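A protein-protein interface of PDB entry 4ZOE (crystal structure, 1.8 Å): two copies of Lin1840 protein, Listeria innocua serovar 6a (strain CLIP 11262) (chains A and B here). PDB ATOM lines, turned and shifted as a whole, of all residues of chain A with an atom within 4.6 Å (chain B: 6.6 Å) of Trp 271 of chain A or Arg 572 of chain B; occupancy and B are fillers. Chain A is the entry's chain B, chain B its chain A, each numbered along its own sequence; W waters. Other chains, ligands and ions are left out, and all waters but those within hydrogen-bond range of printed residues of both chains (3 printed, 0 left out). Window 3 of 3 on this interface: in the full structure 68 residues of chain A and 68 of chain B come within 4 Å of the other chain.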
ATOM      1  N   SER A  26      12.931  21.718  31.385  1.00  0.00           N
ATOM      2  CA  SER A  26      12.930  23.097  31.839  1.00  0.00           C
ATOM      3  C   SER A  26      11.566  23.368  32.529  1.00  0.00           C
ATOM      4  O   SER A  26      10.617  22.702  32.148  1.00  0.00           O
ATOM      5  CB  SER A  26      13.068  24.027  30.624  1.00  0.00           C
ATOM      6  OG  SER A  26      14.447  23.979  30.130  1.00  0.00           O
ATOM      7  N   LEU A  61      14.867  21.156  35.612  1.00  0.00           N
ATOM      8  CA  LEU A  61      16.177  21.830  35.603  1.00  0.00           C
ATOM      9  C   LEU A  61      15.916  23.319  35.507  1.00  0.00           C
ATOM     10  O   LEU A  61      15.251  23.749  34.591  1.00  0.00           O
ATOM     11  CB  LEU A  61      16.891  21.376  34.365  1.00  0.00           C
ATOM     12  CG  LEU A  61      17.979  22.098  33.615  1.00  0.00           C
ATOM     13  CD1 LEU A  61      19.285  21.352  33.699  1.00  0.00           C
ATOM     14  CD2 LEU A  61      17.564  21.973  32.175  1.00  0.00           C
ATOM     15  N   TYR A 205      33.935  21.990  23.058  1.00  0.00           N
ATOM     16  CA  TYR A 205      33.308  20.694  22.715  1.00  0.00           C
ATOM     17  C   TYR A 205      34.250  19.833  21.883  1.00  0.00           C
ATOM     18  O   TYR A 205      33.914  18.735  21.432  1.00  0.00           O
ATOM     19  CB  TYR A 205      32.005  20.818  21.994  1.00  0.00           C
ATOM     20  CG  TYR A 205      31.036  21.823  22.599  1.00  0.00           C
ATOM     21  CD1 TYR A 205      30.552  21.678  23.882  1.00  0.00           C
ATOM     22  CD2 TYR A 205      30.662  22.976  21.859  1.00  0.00           C
ATOM     23  CE1 TYR A 205      29.628  22.592  24.422  1.00  0.00           C
ATOM     24  CE2 TYR A 205      29.702  23.876  22.374  1.00  0.00           C
ATOM     25  CZ  TYR A 205      29.259  23.708  23.678  1.00  0.00           C
ATOM     26  OH  TYR A 205      28.339  24.612  24.210  1.00  0.00           O
ATOM     27  N   PHE A 238      30.458  16.281  27.409  1.00  0.00           N
ATOM     28  CA  PHE A 238      30.234  16.472  25.976  1.00  0.00           C
ATOM     29  C   PHE A 238      31.318  15.855  25.038  1.00  0.00           C
ATOM     30  O   PHE A 238      31.007  15.595  23.896  1.00  0.00           O
ATOM     31  CB  PHE A 238      30.157  17.941  25.581  1.00  0.00           C
ATOM     32  CG  PHE A 238      28.898  18.641  26.022  1.00  0.00           C
ATOM     33  CD1 PHE A 238      27.678  18.059  25.810  1.00  0.00           C
ATOM     34  CD2 PHE A 238      28.977  19.866  26.673  1.00  0.00           C
ATOM     35  CE1 PHE A 238      26.536  18.733  26.201  1.00  0.00           C
ATOM     36  CE2 PHE A 238      27.837  20.541  27.075  1.00  0.00           C
ATOM     37  CZ  PHE A 238      26.631  19.977  26.831  1.00  0.00           C
ATOM     38  N   SER A 269      22.935  13.123  32.045  1.00  0.00           N
ATOM     39  CA  SER A 269      23.627  13.665  30.870  1.00  0.00           C
ATOM     40  C   SER A 269      23.806  15.128  31.016  1.00  0.00           C
ATOM     41  O   SER A 269      23.036  15.824  31.693  1.00  0.00           O
ATOM     42  CB  SER A 269      22.930  13.414  29.547  1.00  0.00           C
ATOM     43  OG  SER A 269      21.739  14.207  29.377  1.00  0.00           O
ATOM     44  N   ASP A 270      24.808  15.625  30.331  1.00  0.00           N
ATOM     45  CA  ASP A 270      24.942  17.062  30.129  1.00  0.00           C
ATOM     46  C   ASP A 270      23.796  17.428  29.158  1.00  0.00           C
ATOM     47  O   ASP A 270      23.072  16.542  28.635  1.00  0.00           O
ATOM     48  CB  ASP A 270      26.373  17.428  29.633  1.00  0.00           C
ATOM     49  CG  ASP A 270      26.792  18.885  29.983  1.00  0.00           C
ATOM     50  OD1 ASP A 270      25.880  19.705  30.141  1.00  0.00           O
ATOM     51  OD2 ASP A 270      28.015  19.218  30.074  1.00  0.00           O
ATOM     52  N   TRP A 271      23.617  18.699  28.911  1.00  0.00           N
ATOM     53  CA  TRP A 271      22.525  19.182  28.095  1.00  0.00           C
ATOM     54  C   TRP A 271      22.492  18.722  26.623  1.00  0.00           C
ATOM     55  O   TRP A 271      23.378  19.077  25.800  1.00  0.00           O
ATOM     56  CB  TRP A 271      22.477  20.710  28.175  1.00  0.00           C
ATOM     57  CG  TRP A 271      21.300  21.284  27.492  1.00  0.00           C
ATOM     58  CD1 TRP A 271      21.043  21.210  26.155  1.00  0.00           C
ATOM     59  CD2 TRP A 271      20.210  22.030  28.048  1.00  0.00           C
ATOM     60  NE1 TRP A 271      19.915  21.862  25.844  1.00  0.00           N
ATOM     61  CE2 TRP A 271      19.370  22.379  26.983  1.00  0.00           C
ATOM     62  CE3 TRP A 271      19.902  22.485  29.309  1.00  0.00           C
ATOM     63  CZ2 TRP A 271      18.211  23.130  27.141  1.00  0.00           C
ATOM     64  CZ3 TRP A 271      18.712  23.244  29.470  1.00  0.00           C
ATOM     65  CH2 TRP A 271      17.901  23.543  28.392  1.00  0.00           C
ATOM     66  N   GLY A 272      21.511  17.889  26.311  1.00  0.00           N
ATOM     67  CA  GLY A 272      21.391  17.308  25.004  1.00  0.00           C
ATOM     68  C   GLY A 272      22.443  16.296  24.659  1.00  0.00           C
ATOM     69  O   GLY A 272      22.462  15.806  23.514  1.00  0.00           O
ATOM     70  N   ALA A 273      23.243  15.888  25.654  1.00  0.00           N
ATOM     71  CA  ALA A 273      24.437  15.075  25.359  1.00  0.00           C
ATOM     72  C   ALA A 273      24.032  13.686  24.852  1.00  0.00           C
ATOM     73  O   ALA A 273      24.781  13.025  24.135  1.00  0.00           O
ATOM     74  CB  ALA A 273      25.368  14.990  26.558  1.00  0.00           C
ATOM     75  N   GLU A 276      23.180  14.160  21.186  1.00  0.00           N
ATOM     76  CA  GLU A 276      24.366  14.684  20.456  1.00  0.00           C
ATOM     77  C   GLU A 276      25.377  13.619  20.191  1.00  0.00           C
ATOM     78  O   GLU A 276      26.237  13.882  19.369  1.00  0.00           O
ATOM     79  CB  GLU A 276      25.001  15.822  21.220  1.00  0.00           C
ATOM     80  CG  GLU A 276      24.248  17.094  21.176  1.00  0.00           C
ATOM     81  CD  GLU A 276      24.703  18.145  22.142  1.00  0.00           C
ATOM     82  OE1 GLU A 276      25.820  18.114  22.688  1.00  0.00           O
ATOM     83  OE2 GLU A 276      23.970  19.123  22.235  1.00  0.00           O
ATOM     84  N   MET A 302      19.056  14.988  29.941  1.00  0.00           N
ATOM     85  CA  MET A 302      18.772  16.423  30.078  1.00  0.00           C
ATOM     86  C   MET A 302      18.238  17.107  28.821  1.00  0.00           C
ATOM     87  O   MET A 302      18.966  17.398  27.880  1.00  0.00           O
ATOM     88  CB  MET A 302      20.009  17.176  30.558  1.00  0.00           C
ATOM     89  CG  MET A 302      19.791  18.660  30.909  1.00  0.00           C
ATOM     90  SD  MET A 302      21.314  19.411  31.436  1.00  0.00           S
ATOM     91  CE  MET A 302      21.664  18.730  33.037  1.00  0.00           C
ATOM     92  N   MET A 303      16.911  17.368  28.827  1.00  0.00           N
ATOM     93  CA  MET A 303      16.268  18.172  27.809  1.00  0.00           C
ATOM     94  C   MET A 303      16.359  17.709  26.335  1.00  0.00           C
ATOM     95  O   MET A 303      16.190  18.493  25.406  1.00  0.00           O
ATOM     96  CB  MET A 303      16.655  19.679  27.967  1.00  0.00           C
ATOM     97  CG  MET A 303      15.851  20.504  28.919  1.00  0.00           C
ATOM     98  SD  MET A 303      14.150  20.648  28.330  1.00  0.00           S
ATOM     99  CE  MET A 303      14.250  21.956  27.108  1.00  0.00           C
ATOM    100  N   GLU A 473      31.185  28.674  29.082  1.00  0.00           N
ATOM    101  CA  GLU A 473      30.893  27.724  28.014  1.00  0.00           C
ATOM    102  C   GLU A 473      30.765  28.424  26.643  1.00  0.00           C
ATOM    103  O   GLU A 473      30.080  29.482  26.465  1.00  0.00           O
ATOM    104  CB  GLU A 473      29.614  26.929  28.285  1.00  0.00           C
ATOM    105  CG  GLU A 473      29.240  25.914  27.175  1.00  0.00           C
ATOM    106  CD  GLU A 473      27.923  25.157  27.499  1.00  0.00           C
ATOM    107  OE1 GLU A 473      27.312  25.495  28.555  1.00  0.00           O
ATOM    108  OE2 GLU A 473      27.551  24.263  26.702  1.00  0.00           O
ATOM    109  N   ARG B 569      33.918  15.279  14.300  1.00  0.00           N
ATOM    110  CA  ARG B 569      32.832  16.202  14.207  1.00  0.00           C
ATOM    111  C   ARG B 569      32.460  16.989  15.449  1.00  0.00           C
ATOM    112  O   ARG B 569      31.893  18.072  15.308  1.00  0.00           O
ATOM    113  CB  ARG B 569      31.664  15.406  13.660  1.00  0.00           C
ATOM    114  CG  ARG B 569      30.464  16.201  13.236  1.00  0.00           C
ATOM    115  CD  ARG B 569      29.792  15.479  12.046  1.00  0.00           C
ATOM    116  NE  ARG B 569      28.777  16.328  11.493  1.00  0.00           N
ATOM    117  CZ  ARG B 569      27.513  16.379  11.898  1.00  0.00           C
ATOM    118  NH1 ARG B 569      27.058  15.662  12.900  1.00  0.00           N
ATOM    119  NH2 ARG B 569      26.697  17.244  11.327  1.00  0.00           N
ATOM    120  N   THR B 570      32.660  16.397  16.645  1.00  0.00           N
ATOM    121  CA  THR B 570      32.144  16.832  17.908  1.00  0.00           C
ATOM    122  C   THR B 570      30.618  16.608  18.018  1.00  0.00           C
ATOM    123  O   THR B 570      29.935  16.255  17.055  1.00  0.00           O
ATOM    124  CB  THR B 570      32.474  18.319  18.328  1.00  0.00           C
ATOM    125  OG1 THR B 570      31.507  19.200  17.801  1.00  0.00           O
ATOM    126  CG2 THR B 570      33.933  18.807  17.909  1.00  0.00           C
ATOM    127  N   GLY B 571      30.150  16.834  19.234  1.00  0.00           N
ATOM    128  CA  GLY B 571      28.710  16.780  19.537  1.00  0.00           C
ATOM    129  C   GLY B 571      27.941  17.977  19.089  1.00  0.00           C
ATOM    130  O   GLY B 571      26.688  17.881  19.012  1.00  0.00           O
ATOM    131  N   ARG B 572      28.631  19.089  18.798  1.00  0.00           N
ATOM    132  CA  ARG B 572      27.956  20.372  18.450  1.00  0.00           C
ATOM    133  C   ARG B 572      28.716  21.085  17.286  1.00  0.00           C
ATOM    134  O   ARG B 572      29.211  22.238  17.407  1.00  0.00           O
ATOM    135  CB  ARG B 572      27.795  21.248  19.675  1.00  0.00           C
ATOM    136  CG  ARG B 572      27.120  20.585  20.880  1.00  0.00           C
ATOM    137  CD  ARG B 572      27.017  21.521  22.025  1.00  0.00           C
ATOM    138  NE  ARG B 572      25.984  21.098  22.956  1.00  0.00           N
ATOM    139  CZ  ARG B 572      25.458  21.844  23.905  1.00  0.00           C
ATOM    140  NH1 ARG B 572      25.824  23.094  24.089  1.00  0.00           N
ATOM    141  NH2 ARG B 572      24.522  21.331  24.696  1.00  0.00           N
ATOM    142  N   PRO B 573      28.768  20.433  16.152  1.00  0.00           N
ATOM    143  CA  PRO B 573      29.363  20.984  14.957  1.00  0.00           C
ATOM    144  C   PRO B 573      28.737  22.265  14.505  1.00  0.00           C
ATOM    145  O   PRO B 573      27.508  22.467  14.675  1.00  0.00           O
ATOM    146  CB  PRO B 573      29.136  19.865  13.901  1.00  0.00           C
ATOM    147  CG  PRO B 573      27.968  19.158  14.395  1.00  0.00           C
ATOM    148  CD  PRO B 573      28.050  19.147  15.873  1.00  0.00           C
ATOM    149  N   GLN B 574      29.582  23.144  14.025  1.00  0.00           N
ATOM    150  CA  GLN B 574      29.164  24.335  13.351  1.00  0.00           C
ATOM    151  C   GLN B 574      28.666  23.901  11.975  1.00  0.00           C
ATOM    152  O   GLN B 574      29.263  23.052  11.282  1.00  0.00           O
ATOM    153  CB  GLN B 574      30.336  25.366  13.341  1.00  0.00           C
ATOM    154  CG  GLN B 574      29.907  26.750  13.236  1.00  0.00           C
ATOM    155  CD  GLN B 574      31.032  27.746  12.996  1.00  0.00           C
ATOM    156  OE1 GLN B 574      31.931  27.578  12.138  1.00  0.00           O
ATOM    157  NE2 GLN B 574      30.988  28.803  13.755  1.00  0.00           N
ATOM    158  N   THR B 575      27.475  24.361  11.654  1.00  0.00           N
ATOM    159  CA  THR B 575      26.873  24.069  10.385  1.00  0.00           C
ATOM    160  C   THR B 575      26.545  25.413   9.735  1.00  0.00           C
ATOM    161  O   THR B 575      26.638  26.489  10.382  1.00  0.00           O
ATOM    162  CB  THR B 575      25.604  23.207  10.536  1.00  0.00           C
ATOM    163  OG1 THR B 575      24.647  23.905  11.308  1.00  0.00           O
ATOM    164  CG2 THR B 575      25.901  21.872  11.238  1.00  0.00           C
ATOM    165  N   ASN B 578      23.480  26.770  11.774  1.00  0.00           N
ATOM    166  CA  ASN B 578      23.552  27.286  13.184  1.00  0.00           C
ATOM    167  C   ASN B 578      24.583  28.412  13.374  1.00  0.00           C
ATOM    168  O   ASN B 578      24.861  28.796  14.493  1.00  0.00           O
ATOM    169  CB  ASN B 578      23.767  26.173  14.225  1.00  0.00           C
ATOM    170  CG  ASN B 578      25.110  25.478  14.098  1.00  0.00           C
ATOM    171  OD1 ASN B 578      26.093  26.043  13.641  1.00  0.00           O
ATOM    172  ND2 ASN B 578      25.156  24.226  14.542  1.00  0.00           N
ATOM    173  N   TYR B 583      26.137  28.223  21.412  1.00  0.00           N
ATOM    174  CA  TYR B 583      26.377  26.902  22.018  1.00  0.00           C
ATOM    175  C   TYR B 583      26.700  25.873  20.892  1.00  0.00           C
ATOM    176  O   TYR B 583      26.003  24.850  20.672  1.00  0.00           O
ATOM    177  CB  TYR B 583      25.208  26.517  22.919  1.00  0.00           C
ATOM    178  CG  TYR B 583      25.171  27.391  24.125  1.00  0.00           C
ATOM    179  CD1 TYR B 583      26.211  27.358  25.062  1.00  0.00           C
ATOM    180  CD2 TYR B 583      24.163  28.346  24.293  1.00  0.00           C
ATOM    181  CE1 TYR B 583      26.259  28.223  26.109  1.00  0.00           C
ATOM    182  CE2 TYR B 583      24.203  29.223  25.369  1.00  0.00           C
ATOM    183  CZ  TYR B 583      25.237  29.142  26.268  1.00  0.00           C
ATOM    184  OH  TYR B 583      25.308  30.003  27.317  1.00  0.00           O
ATOM    185  N   VAL B 584      27.804  26.167  20.192  1.00  0.00           N
ATOM    186  CA  VAL B 584      28.331  25.322  19.134  1.00  0.00           C
ATOM    187  C   VAL B 584      29.866  25.419  19.210  1.00  0.00           C
ATOM    188  O   VAL B 584      30.438  26.335  19.823  1.00  0.00           O
ATOM    189  CB  VAL B 584      27.885  25.751  17.678  1.00  0.00           C
ATOM    190  CG1 VAL B 584      26.373  25.787  17.480  1.00  0.00           C
ATOM    191  CG2 VAL B 584      28.442  27.078  17.245  1.00  0.00           C
ATOM    192  N   SER B 585      30.519  24.444  18.596  1.00  0.00           N
ATOM    193  CA  SER B 585      31.990  24.415  18.617  1.00  0.00           C
ATOM    194  C   SER B 585      32.607  25.515  17.714  1.00  0.00           C
ATOM    195  O   SER B 585      32.523  25.447  16.469  1.00  0.00           O
ATOM    196  CB  SER B 585      32.413  23.047  18.155  1.00  0.00           C
ATOM    197  OG  SER B 585      33.824  22.895  18.211  1.00  0.00           O
ATOM    198  N   HIS B 586      33.105  26.588  18.337  1.00  0.00           N
ATOM    199  CA  HIS B 586      33.662  27.699  17.596  1.00  0.00           C
ATOM    200  C   HIS B 586      34.554  28.494  18.524  1.00  0.00           C
ATOM    201  O   HIS B 586      34.583  28.283  19.731  1.00  0.00           O
ATOM    202  CB  HIS B 586      32.496  28.629  17.061  1.00  0.00           C
ATOM    203  CG  HIS B 586      31.848  29.507  18.098  1.00  0.00           C
ATOM    204  ND1 HIS B 586      31.080  29.017  19.131  1.00  0.00           N
ATOM    205  CD2 HIS B 586      31.779  30.864  18.207  1.00  0.00           C
ATOM    206  CE1 HIS B 586      30.638  30.027  19.879  1.00  0.00           C
ATOM    207  NE2 HIS B 586      31.065  31.156  19.348  1.00  0.00           N
HETATM  208  O   HOH W   1      24.748  23.568  26.768  1.00  0.00           O
HETATM  209  O   HOH W   2      28.233  30.723  27.970  1.00  0.00           O
HETATM  210  O   HOH W   3      31.397  17.429  21.742  1.00  0.00           O
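The guanidinium group (NH1) of Arg 572 of chain B lies within hydrogen-bond range of the side-chain hydroxyl (OH) of Tyr 205 of chain A.
The guanidinium group (NH2) of Arg 572 of chain B sits at hydrogen-bond distance from the backbone carbonyl oxygen (O) of Trp 271 of chain A, 2.8 Å away.
The guanidinium group (NE) of Arg 572 of chain B is in salt-bridge range of the side-chain carboxylate (OE2) of Glu 276 of chain A (2.9 Å).
NH1 of Arg 572 of chain B lies within salt-bridge range of OE2 of Glu 473 of chain A, 3.3 Å away.
The side-chain hydroxyl (OG1) of Thr 570 of chain B is in hydrogen-bond range of the backbone NH (N) of Arg 572 of chain B (3.0 Å).
The backbone NH (N) of Ser 585 of chain B is in hydrogen-bond range of the backbone carbonyl oxygen (O) of Arg 572 of chain B, at 2.8 Å.
ND1 of His 586 of chain B sits at hydrogen-bond distance from O of Val 584 of chain B, at 2.8 Å.
OH of Tyr 205 of chain A is in hydrogen-bond range of OE2 of Glu 473 of chain A, at 2.6 Å.
N of Trp 271 of chain A is in hydrogen-bond range of SD of Met 302 of chain A, at 3.5 Å.
Among the printed residues, pairs that only touch across the chains: Phe 238 of chain A with Arg 572 of chain B, Glu 276 of chain A with Gly 571 of chain B, Tyr 205 of chain A with Thr 570 of chain B, Tyr 205 of chain A with Val 584 of chain B, Tyr 205 of chain A with Tyr 583 of chain B, Tyr 205 of chain A with Ser 585 of chain B and Glu 473 of chain A with Tyr 583 of chain B.
Of chain A, only Tyr 205, Phe 238, Trp 271, Glu 276 and Glu 473 come within 4 Å of Arg 572 of chain B.
Of the printed residues of chain B, Tyr 205 of chain A touches Thr 570 (3.4 Å), Arg 572 (2.9 Å), Tyr 583 (3.6 Å), Val 584 (3.5 Å) and Ser 585 (3.6 Å).
Printed residues of chain A within 4 Å of Gly 571 of chain B: Glu 276.
Printed residues of chain A within 4 Å of Val 584 of chain B: Tyr 205 (3.5 Å).
Of the printed residues of chain A, Ser 585 of chain B touches Tyr 205.
Of the printed residues of chain B, Glu 473 of chain A touches Arg 572 and Tyr 583.
The nearest printed residue of chain A that does not touch Arg 572 of chain B is Gly 272 of chain A (4.8 Å).
The nearest printed residue of chain A that does not touch Gly 571 of chain B is Tyr 205 of chain A (4.8 Å).
Printed residues of chain B that touch a printed residue of chain A: Thr 570, Gly 571, Arg 572, Tyr 583, Val 584 and Ser 585.
Of the 13 printed residues of chain A, 5 touch a printed residue of chain B.
Among the printed residues, 11 pairs touch across the chains.
Among the printed residues, Asp or Glu carboxylates within 4 Å of a Lys or Arg side-chain nitrogen of the other chain: Glu 276 of chain A with Arg 572 of chain B and Glu 473 of chain A with Arg 572 of chain B.
No position is printed for both chains.
Of the 11 pairs that touch across the chains among the printed residues, none has its exchanged pair printed and touching as well.
Water W2 bridges the backbone carbonyl oxygen (O) of Glu 473 of chain A and the side-chain hydroxyl (OH) of Tyr 583 of chain B.
Water W3 lies within hydrogen-bond range of O of Tyr 205 of chain A, O of Phe 238 of chain A and N of Gly 571 of chain B.
Water W1 lies within hydrogen-bond range of the side-chain carboxylate of Glu 473 of chain A (2.9 Å) and the guanidinium group of Arg 572 of chain B (2.9 Å).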
